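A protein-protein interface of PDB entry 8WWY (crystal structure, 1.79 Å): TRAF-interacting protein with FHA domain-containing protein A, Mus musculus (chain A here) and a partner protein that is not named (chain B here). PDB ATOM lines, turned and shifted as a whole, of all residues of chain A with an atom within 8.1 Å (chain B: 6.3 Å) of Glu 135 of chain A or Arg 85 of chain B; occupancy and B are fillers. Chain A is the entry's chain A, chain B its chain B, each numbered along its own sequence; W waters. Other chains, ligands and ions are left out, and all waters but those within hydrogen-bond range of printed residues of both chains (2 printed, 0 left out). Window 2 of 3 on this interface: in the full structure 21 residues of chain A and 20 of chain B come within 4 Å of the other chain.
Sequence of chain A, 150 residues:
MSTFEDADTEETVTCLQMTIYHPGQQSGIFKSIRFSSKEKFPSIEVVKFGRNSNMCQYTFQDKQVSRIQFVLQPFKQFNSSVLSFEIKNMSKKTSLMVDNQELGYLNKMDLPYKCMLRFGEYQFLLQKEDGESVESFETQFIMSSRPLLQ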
ATOM      1  N   GLU A  11      25.639 -28.592  27.391  1.00  0.00           N
ATOM      2  CA  GLU A  11      26.505 -28.352  26.239  1.00  0.00           C
ATOM      3  C   GLU A  11      27.547 -27.274  26.534  1.00  0.00           C
ATOM      4  O   GLU A  11      27.253 -26.301  27.217  1.00  0.00           O
ATOM      5  CB  GLU A  11      25.667 -27.947  25.019  1.00  0.00           C
ATOM      6  CG  GLU A  11      24.817 -29.078  24.461  1.00  0.00           C
ATOM      7  CD  GLU A  11      25.335 -29.601  23.135  1.00  0.00           C
ATOM      8  OE1 GLU A  11      25.028 -28.970  22.108  1.00  0.00           O
ATOM      9  OE2 GLU A  11      26.049 -30.628  23.116  1.00  0.00           O
ATOM     10  N   THR A  12      28.766 -27.475  26.029  1.00  0.00           N
ATOM     11  CA  THR A  12      29.786 -26.439  26.067  1.00  0.00           C
ATOM     12  C   THR A  12      29.322 -25.217  25.271  1.00  0.00           C
ATOM     13  O   THR A  12      28.429 -25.295  24.418  1.00  0.00           O
ATOM     14  CB  THR A  12      31.097 -26.955  25.489  1.00  0.00           C
ATOM     15  OG1 THR A  12      30.853 -27.491  24.188  1.00  0.00           O
ATOM     16  CG2 THR A  12      31.673 -28.047  26.372  1.00  0.00           C
ATOM     17  N   VAL A  13      29.944 -24.074  25.550  1.00  0.00           N
ATOM     18  CA  VAL A  13      29.544 -22.794  24.969  1.00  0.00           C
ATOM     19  C   VAL A  13      30.758 -22.164  24.300  1.00  0.00           C
ATOM     20  O   VAL A  13      31.827 -22.072  24.910  1.00  0.00           O
ATOM     21  CB  VAL A  13      28.971 -21.847  26.042  1.00  0.00           C
ATOM     22  CG1 VAL A  13      28.598 -20.505  25.430  1.00  0.00           C
ATOM     23  CG2 VAL A  13      27.776 -22.486  26.734  1.00  0.00           C
ATOM     24  N   LYS A  40      27.274 -14.536  29.248  1.00  0.00           N
ATOM     25  CA  LYS A  40      26.544 -15.283  28.233  1.00  0.00           C
ATOM     26  C   LYS A  40      25.563 -14.385  27.484  1.00  0.00           C
ATOM     27  O   LYS A  40      24.864 -13.566  28.086  1.00  0.00           O
ATOM     28  CB  LYS A  40      25.806 -16.457  28.882  1.00  0.00           C
ATOM     29  CG  LYS A  40      25.159 -17.407  27.894  1.00  0.00           C
ATOM     30  CD  LYS A  40      24.625 -18.647  28.592  1.00  0.00           C
ATOM     31  CE  LYS A  40      25.763 -19.544  29.058  1.00  0.00           C
ATOM     32  NZ  LYS A  40      25.264 -20.819  29.654  1.00  0.00           N
ATOM     33  N   PHE A  41      25.524 -14.543  26.160  1.00  0.00           N
ATOM     34  CA  PHE A  41      24.603 -13.835  25.282  1.00  0.00           C
ATOM     35  C   PHE A  41      23.833 -14.832  24.430  1.00  0.00           C
ATOM     36  O   PHE A  41      24.400 -15.845  24.009  1.00  0.00           O
ATOM     37  CB  PHE A  41      25.338 -12.872  24.340  1.00  0.00           C
ATOM     38  CG  PHE A  41      26.043 -11.753  25.040  1.00  0.00           C
ATOM     39  CD1 PHE A  41      25.379 -10.568  25.324  1.00  0.00           C
ATOM     40  CD2 PHE A  41      27.372 -11.878  25.402  1.00  0.00           C
ATOM     41  CE1 PHE A  41      26.027  -9.533  25.963  1.00  0.00           C
ATOM     42  CE2 PHE A  41      28.025 -10.843  26.050  1.00  0.00           C
ATOM     43  CZ  PHE A  41      27.349  -9.666  26.325  1.00  0.00           C
ATOM     44  N   PRO A  42      22.558 -14.573  24.147  1.00  0.00           N
ATOM     45  CA  PRO A  42      21.879 -15.331  23.086  1.00  0.00           C
ATOM     46  C   PRO A  42      22.591 -15.097  21.768  1.00  0.00           C
ATOM     47  O   PRO A  42      23.072 -13.996  21.498  1.00  0.00           O
ATOM     48  CB  PRO A  42      20.461 -14.742  23.065  1.00  0.00           C
ATOM     49  CG  PRO A  42      20.340 -13.905  24.301  1.00  0.00           C
ATOM     50  CD  PRO A  42      21.724 -13.483  24.680  1.00  0.00           C
ATOM     51  N   SER A  43      22.656 -16.144  20.937  1.00  0.00           N
ATOM     52  CA  SER A  43      23.325 -16.003  19.648  1.00  0.00           C
ATOM     53  C   SER A  43      22.548 -15.141  18.658  1.00  0.00           C
ATOM     54  O   SER A  43      23.071 -14.865  17.574  1.00  0.00           O
ATOM     55  CB  SER A  43      23.610 -17.378  19.032  1.00  0.00           C
ATOM     56  OG  SER A  43      22.484 -18.238  19.086  1.00  0.00           O
ATOM     57  N   ILE A  44      21.337 -14.701  19.002  1.00  0.00           N
ATOM     58  CA  ILE A  44      20.598 -13.747  18.172  1.00  0.00           C
ATOM     59  C   ILE A  44      20.856 -12.325  18.651  1.00  0.00           C
ATOM     60  O   ILE A  44      20.246 -11.372  18.151  1.00  0.00           O
ATOM     61  CB  ILE A  44      19.087 -14.025  18.169  1.00  0.00           C
ATOM     62  CG1 ILE A  44      18.526 -13.929  19.591  1.00  0.00           C
ATOM     63  CG2 ILE A  44      18.779 -15.367  17.510  1.00  0.00           C
ATOM     64  CD1 ILE A  44      17.006 -13.843  19.637  1.00  0.00           C
ATOM     65  N   GLU A  45      21.739 -12.161  19.626  1.00  0.00           N
ATOM     66  CA  GLU A  45      22.119 -10.820  20.046  1.00  0.00           C
ATOM     67  C   GLU A  45      23.310 -10.341  19.222  1.00  0.00           C
ATOM     68  O   GLU A  45      24.074 -11.136  18.683  1.00  0.00           O
ATOM     69  CB  GLU A  45      22.462 -10.789  21.539  1.00  0.00           C
ATOM     70  CG  GLU A  45      22.537  -9.391  22.124  1.00  0.00           C
ATOM     71  CD  GLU A  45      21.285  -8.587  21.841  1.00  0.00           C
ATOM     72  OE1 GLU A  45      20.209  -8.970  22.346  1.00  0.00           O
ATOM     73  OE2 GLU A  45      21.372  -7.587  21.097  1.00  0.00           O
ATOM     74  N   LYS A  76      26.123 -18.508  11.171  1.00  0.00           N
ATOM     75  CA  LYS A  76      26.569 -19.868  10.864  1.00  0.00           C
ATOM     76  C   LYS A  76      26.814 -20.005   9.372  1.00  0.00           C
ATOM     77  O   LYS A  76      25.942 -19.667   8.567  1.00  0.00           O
ATOM     78  CB  LYS A  76      25.546 -20.912  11.334  1.00  0.00           C
ATOM     79  CG  LYS A  76      25.560 -21.126  12.850  1.00  0.00           C
ATOM     80  CD  LYS A  76      24.548 -22.165  13.297  1.00  0.00           C
ATOM     81  CE  LYS A  76      25.020 -23.583  12.984  1.00  0.00           C
ATOM     82  NZ  LYS A  76      24.079 -24.303  12.077  1.00  0.00           N
ATOM     83  N   LEU A  83      29.603 -21.875  15.621  1.00  0.00           N
ATOM     84  CA  LEU A  83      29.197 -20.479  15.590  1.00  0.00           C
ATOM     85  C   LEU A  83      30.355 -19.612  15.103  1.00  0.00           C
ATOM     86  O   LEU A  83      31.426 -19.600  15.720  1.00  0.00           O
ATOM     87  CB  LEU A  83      28.750 -20.061  16.986  1.00  0.00           C
ATOM     88  CG  LEU A  83      28.125 -18.696  17.195  1.00  0.00           C
ATOM     89  CD1 LEU A  83      26.902 -18.513  16.295  1.00  0.00           C
ATOM     90  CD2 LEU A  83      27.754 -18.545  18.670  1.00  0.00           C
ATOM     91  N   GLU A 132      29.665 -26.278  21.752  1.00  0.00           N
ATOM     92  CA  GLU A 132      28.601 -26.976  21.042  1.00  0.00           C
ATOM     93  C   GLU A 132      27.251 -26.273  21.105  1.00  0.00           C
ATOM     94  O   GLU A 132      26.375 -26.573  20.285  1.00  0.00           O
ATOM     95  CB  GLU A 132      28.466 -28.399  21.585  1.00  0.00           C
ATOM     96  CG  GLU A 132      29.604 -29.305  21.126  1.00  0.00           C
ATOM     97  CD  GLU A 132      29.740 -29.323  19.608  1.00  0.00           C
ATOM     98  OE1 GLU A 132      28.746 -29.644  18.926  1.00  0.00           O
ATOM     99  OE2 GLU A 132      30.833 -28.997  19.098  1.00  0.00           O
ATOM    100  N   SER A 133      27.048 -25.363  22.048  1.00  0.00           N
ATOM    101  CA  SER A 133      25.788 -24.637  22.092  1.00  0.00           C
ATOM    102  C   SER A 133      25.609 -23.811  20.824  1.00  0.00           C
ATOM    103  O   SER A 133      26.543 -23.159  20.351  1.00  0.00           O
ATOM    104  CB  SER A 133      25.735 -23.734  23.318  1.00  0.00           C
ATOM    105  OG  SER A 133      24.611 -22.871  23.234  1.00  0.00           O
ATOM    106  N   VAL A 134      24.413 -23.861  20.252  1.00  0.00           N
ATOM    107  CA  VAL A 134      24.110 -22.989  19.128  1.00  0.00           C
ATOM    108  C   VAL A 134      23.264 -21.796  19.553  1.00  0.00           C
ATOM    109  O   VAL A 134      23.192 -20.806  18.809  1.00  0.00           O
ATOM    110  CB  VAL A 134      23.421 -23.771  17.989  1.00  0.00           C
ATOM    111  CG1 VAL A 134      22.008 -24.179  18.393  1.00  0.00           C
ATOM    112  CG2 VAL A 134      23.432 -22.969  16.696  1.00  0.00           C
ATOM    113  N   GLU A 135      22.655 -21.841  20.733  1.00  0.00           N
ATOM    114  CA  GLU A 135      21.764 -20.765  21.138  1.00  0.00           C
ATOM    115  C   GLU A 135      22.458 -19.684  21.957  1.00  0.00           C
ATOM    116  O   GLU A 135      21.872 -18.614  22.153  1.00  0.00           O
ATOM    117  CB  GLU A 135      20.583 -21.333  21.927  1.00  0.00           C
ATOM    118  CG  GLU A 135      19.786 -22.364  21.147  1.00  0.00           C
ATOM    119  CD  GLU A 135      18.397 -22.580  21.707  1.00  0.00           C
ATOM    120  OE1 GLU A 135      18.066 -21.958  22.737  1.00  0.00           O
ATOM    121  OE2 GLU A 135      17.634 -23.371  21.111  1.00  0.00           O
ATOM    122  N   SER A 136      23.686 -19.931  22.423  1.00  0.00           N
ATOM    123  CA  SER A 136      24.394 -19.005  23.304  1.00  0.00           C
ATOM    124  C   SER A 136      25.871 -18.939  22.941  1.00  0.00           C
ATOM    125  O   SER A 136      26.425 -19.854  22.328  1.00  0.00           O
ATOM    126  CB  SER A 136      24.288 -19.418  24.785  1.00  0.00           C
ATOM    127  OG  SER A 136      22.945 -19.499  25.206  1.00  0.00           O
ATOM    128  N   PHE A 137      26.512 -17.852  23.373  1.00  0.00           N
ATOM    129  CA  PHE A 137      27.964 -17.747  23.354  1.00  0.00           C
ATOM    130  C   PHE A 137      28.385 -16.887  24.538  1.00  0.00           C
ATOM    131  O   PHE A 137      27.567 -16.180  25.135  1.00  0.00           O
ATOM    132  CB  PHE A 137      28.494 -17.191  22.021  1.00  0.00           C
ATOM    133  CG  PHE A 137      28.138 -15.750  21.767  1.00  0.00           C
ATOM    134  CD1 PHE A 137      26.916 -15.414  21.184  1.00  0.00           C
ATOM    135  CD2 PHE A 137      29.026 -14.737  22.092  1.00  0.00           C
ATOM    136  CE1 PHE A 137      26.583 -14.083  20.942  1.00  0.00           C
ATOM    137  CE2 PHE A 137      28.695 -13.403  21.859  1.00  0.00           C
ATOM    138  CZ  PHE A 137      27.475 -13.081  21.283  1.00  0.00           C
ATOM    139  N   SER B  59       8.812 -16.640  15.283  1.00  0.00           N
ATOM    140  CA  SER B  59       9.542 -16.373  16.511  1.00  0.00           C
ATOM    141  C   SER B  59       9.440 -14.888  16.850  1.00  0.00           C
ATOM    142  O   SER B  59       9.153 -14.055  15.986  1.00  0.00           O
ATOM    143  CB  SER B  59      11.012 -16.773  16.373  1.00  0.00           C
ATOM    144  OG  SER B  59      11.148 -18.166  16.139  1.00  0.00           O
ATOM    145  N   TYR B  61      11.866 -12.977  17.415  1.00  0.00           N
ATOM    146  CA  TYR B  61      12.834 -12.448  16.461  1.00  0.00           C
ATOM    147  C   TYR B  61      12.996 -13.516  15.396  1.00  0.00           C
ATOM    148  O   TYR B  61      13.499 -14.608  15.682  1.00  0.00           O
ATOM    149  CB  TYR B  61      14.160 -12.112  17.140  1.00  0.00           C
ATOM    150  CG  TYR B  61      13.975 -11.172  18.309  1.00  0.00           C
ATOM    151  CD1 TYR B  61      13.916  -9.798  18.117  1.00  0.00           C
ATOM    152  CD2 TYR B  61      13.804 -11.663  19.601  1.00  0.00           C
ATOM    153  CE1 TYR B  61      13.727  -8.933  19.180  1.00  0.00           C
ATOM    154  CE2 TYR B  61      13.612 -10.802  20.675  1.00  0.00           C
ATOM    155  CZ  TYR B  61      13.576  -9.439  20.455  1.00  0.00           C
ATOM    156  OH  TYR B  61      13.389  -8.577  21.512  1.00  0.00           O
ATOM    157  N   VAL B  82      18.703 -15.434   9.338  1.00  0.00           N
ATOM    158  CA  VAL B  82      17.593 -16.110  10.007  1.00  0.00           C
ATOM    159  C   VAL B  82      17.837 -16.143  11.509  1.00  0.00           C
ATOM    160  O   VAL B  82      18.903 -16.571  11.964  1.00  0.00           O
ATOM    161  CB  VAL B  82      17.423 -17.524   9.439  1.00  0.00           C
ATOM    162  CG1 VAL B  82      16.420 -18.334  10.258  1.00  0.00           C
ATOM    163  CG2 VAL B  82      17.001 -17.420   7.989  1.00  0.00           C
ATOM    164  N   LEU B  83      16.842 -15.700  12.290  1.00  0.00           N
ATOM    165  CA  LEU B  83      16.959 -15.674  13.744  1.00  0.00           C
ATOM    166  C   LEU B  83      16.065 -16.693  14.431  1.00  0.00           C
ATOM    167  O   LEU B  83      16.251 -16.949  15.622  1.00  0.00           O
ATOM    168  CB  LEU B  83      16.632 -14.271  14.283  1.00  0.00           C
ATOM    169  CG  LEU B  83      17.508 -13.135  13.770  1.00  0.00           C
ATOM    170  CD1 LEU B  83      17.052 -11.805  14.336  1.00  0.00           C
ATOM    171  CD2 LEU B  83      18.989 -13.382  14.126  1.00  0.00           C
ATOM    172  N   THR B  84      15.113 -17.291  13.714  1.00  0.00           N
ATOM    173  CA  THR B  84      14.231 -18.270  14.318  1.00  0.00           C
ATOM    174  C   THR B  84      14.918 -19.627  14.397  1.00  0.00           C
ATOM    175  O   THR B  84      15.702 -19.999  13.520  1.00  0.00           O
ATOM    176  CB  THR B  84      12.936 -18.399  13.517  1.00  0.00           C
ATOM    177  OG1 THR B  84      12.121 -19.422  14.103  1.00  0.00           O
ATOM    178  CG2 THR B  84      13.240 -18.761  12.060  1.00  0.00           C
ATOM    179  N   ARG B  85      14.624 -20.361  15.469  1.00  0.00           N
ATOM    180  CA  ARG B  85      14.988 -21.771  15.564  1.00  0.00           C
ATOM    181  C   ARG B  85      13.898 -22.690  15.030  1.00  0.00           C
ATOM    182  O   ARG B  85      14.135 -23.892  14.880  1.00  0.00           O
ATOM    183  CB  ARG B  85      15.272 -22.157  17.019  1.00  0.00           C
ATOM    184  CG  ARG B  85      16.366 -21.374  17.693  1.00  0.00           C
ATOM    185  CD  ARG B  85      17.729 -21.980  17.421  1.00  0.00           C
ATOM    186  NE  ARG B  85      18.073 -23.098  18.298  1.00  0.00           N
ATOM    187  CZ  ARG B  85      18.482 -24.290  17.869  1.00  0.00           C
ATOM    188  NH1 ARG B  85      18.601 -24.531  16.568  1.00  0.00           N
ATOM    189  NH2 ARG B  85      18.780 -25.241  18.742  1.00  0.00           N
ATOM    190  N   LYS B  86      12.716 -22.156  14.742  1.00  0.00           N
ATOM    191  CA  LYS B  86      11.531 -22.982  14.547  1.00  0.00           C
ATOM    192  C   LYS B  86      11.349 -23.471  13.117  1.00  0.00           C
ATOM    193  O   LYS B  86      10.749 -24.531  12.909  1.00  0.00           O
ATOM    194  CB  LYS B  86      10.279 -22.209  14.978  1.00  0.00           C
ATOM    195  CG  LYS B  86      10.252 -21.826  16.453  1.00  0.00           C
ATOM    196  CD  LYS B  86       8.833 -21.502  16.924  1.00  0.00           C
ATOM    197  CE  LYS B  86       8.484 -20.027  16.752  1.00  0.00           C
ATOM    198  NZ  LYS B  86       7.030 -19.743  17.023  1.00  0.00           N
ATOM    199  N   SER B  87      11.834 -22.738  12.121  1.00  0.00           N
ATOM    200  CA  SER B  87      11.508 -23.084  10.744  1.00  0.00           C
ATOM    201  C   SER B  87      12.540 -22.462   9.816  1.00  0.00           C
ATOM    202  O   SER B  87      13.427 -21.720  10.247  1.00  0.00           O
ATOM    203  CB  SER B  87      10.092 -22.617  10.400  1.00  0.00           C
ATOM    204  OG  SER B  87       9.838 -21.355  10.999  1.00  0.00           O
ATOM    205  N   TYR B  98      18.537 -21.458  11.070  1.00  0.00           N
ATOM    206  CA  TYR B  98      19.034 -20.619  12.157  1.00  0.00           C
ATOM    207  C   TYR B  98      20.447 -20.100  11.933  1.00  0.00           C
ATOM    208  O   TYR B  98      21.395 -20.887  11.766  1.00  0.00           O
ATOM    209  CB  TYR B  98      18.973 -21.428  13.450  1.00  0.00           C
ATOM    210  CG  TYR B  98      19.324 -20.661  14.693  1.00  0.00           C
ATOM    211  CD1 TYR B  98      18.606 -19.531  15.070  1.00  0.00           C
ATOM    212  CD2 TYR B  98      20.348 -21.100  15.524  1.00  0.00           C
ATOM    213  CE1 TYR B  98      18.915 -18.852  16.235  1.00  0.00           C
ATOM    214  CE2 TYR B  98      20.666 -20.424  16.682  1.00  0.00           C
ATOM    215  CZ  TYR B  98      19.949 -19.311  17.037  1.00  0.00           C
ATOM    216  OH  TYR B  98      20.286 -18.647  18.199  1.00  0.00           O
HETATM  217  O   HOH W   1      19.551 -17.359  20.463  1.00  0.00           O
HETATM  218  O   HOH W   2      21.838 -23.457  11.445  1.00  0.00           O
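The guanidinium group (NE) of Arg 85 of chain B is in salt-bridge range of the side-chain carboxylate (OE2) of Glu 135 of chain A (2.9 Å). The side-chain hydroxyl (OG) of Ser 43 of chain A is in hydrogen-bond range of the side-chain hydroxyl (OH) of Tyr 98 of chain B, at 2.4 Å.
OG of Ser 43 of chain A sits at hydrogen-bond distance from O of Val 134 of chain A (2.7 Å). The backbone NH of Ser 43 of chain A is in hydrogen-bond range of the backbone carbonyl oxygen of Glu 135 of chain A, 2.9 Å away. The backbone NH (N) of Glu 135 of chain A sits at hydrogen-bond distance from the side-chain hydroxyl (OG) of Ser 133 of chain A (3.3 Å).
Among the printed residues, pairs that only touch across the chains: Ile 44 of chain A with Tyr 61 of chain B (3.9 Å), Ile 44 of chain A with Leu 83 of chain B (3.5 Å), Ile 44 of chain A with Tyr 98 of chain B (3.7 Å), Lys 76 of chain A with Tyr 98 of chain B (3.7 Å), Val 134 of chain A with Arg 85 of chain B (3.4 Å), Val 134 of chain A with Tyr 98 of chain B (3.3 Å) and Glu 135 of chain A with Tyr 98 of chain B (3.9 Å).
Pro 42 of chain A touches none of the printed residues of chain B. Printed residues of chain B within 4 Å of Ser 43 of chain A: Tyr 98 (2.4 Å). Glu 135 of chain A touches just these residues of chain B: Arg 85 and Tyr 98. Printed residues of chain A within 4 Å of Leu 83 of chain B: Ile 44. No residue of chain A comes within 4 Å of Thr 84 of chain B. Of chain A, only Val 134 and Glu 135 come within 4 Å of Arg 85 of chain B. Of the printed residues of chain A, Tyr 98 of chain B touches Ser 43 (2.4 Å), Ile 44 (3.7 Å), Lys 76 (3.7 Å), Val 134 (3.3 Å) and Glu 135 (3.9 Å). The nearest printed residue of chain B that does not touch Lys 76 of chain A is Arg 85 of chain B (7.1 Å).
Of the 9 printed residues of chain B, 4 touch a printed residue of chain A. Printed residues of chain B that touch a printed residue of chain A: Tyr 61, Leu 83, Arg 85 and Tyr 98. Along chain B the printed residues that touch a printed residue of chain A span positions 61 to 98. Of the 17 printed residues of chain A, 5 touch a printed residue of chain B. Among the printed residues, 9 pairs touch across the chains.
Water W2 bridges NZ of Lys 76 of chain A (2.5 Å) and O of Tyr 98 of chain B (2.6 Å). Water W1 lies within hydrogen-bond range of OH of Tyr 98 of chain B, O of Glu 135 of chain A and OG of Ser 43 of chain A.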
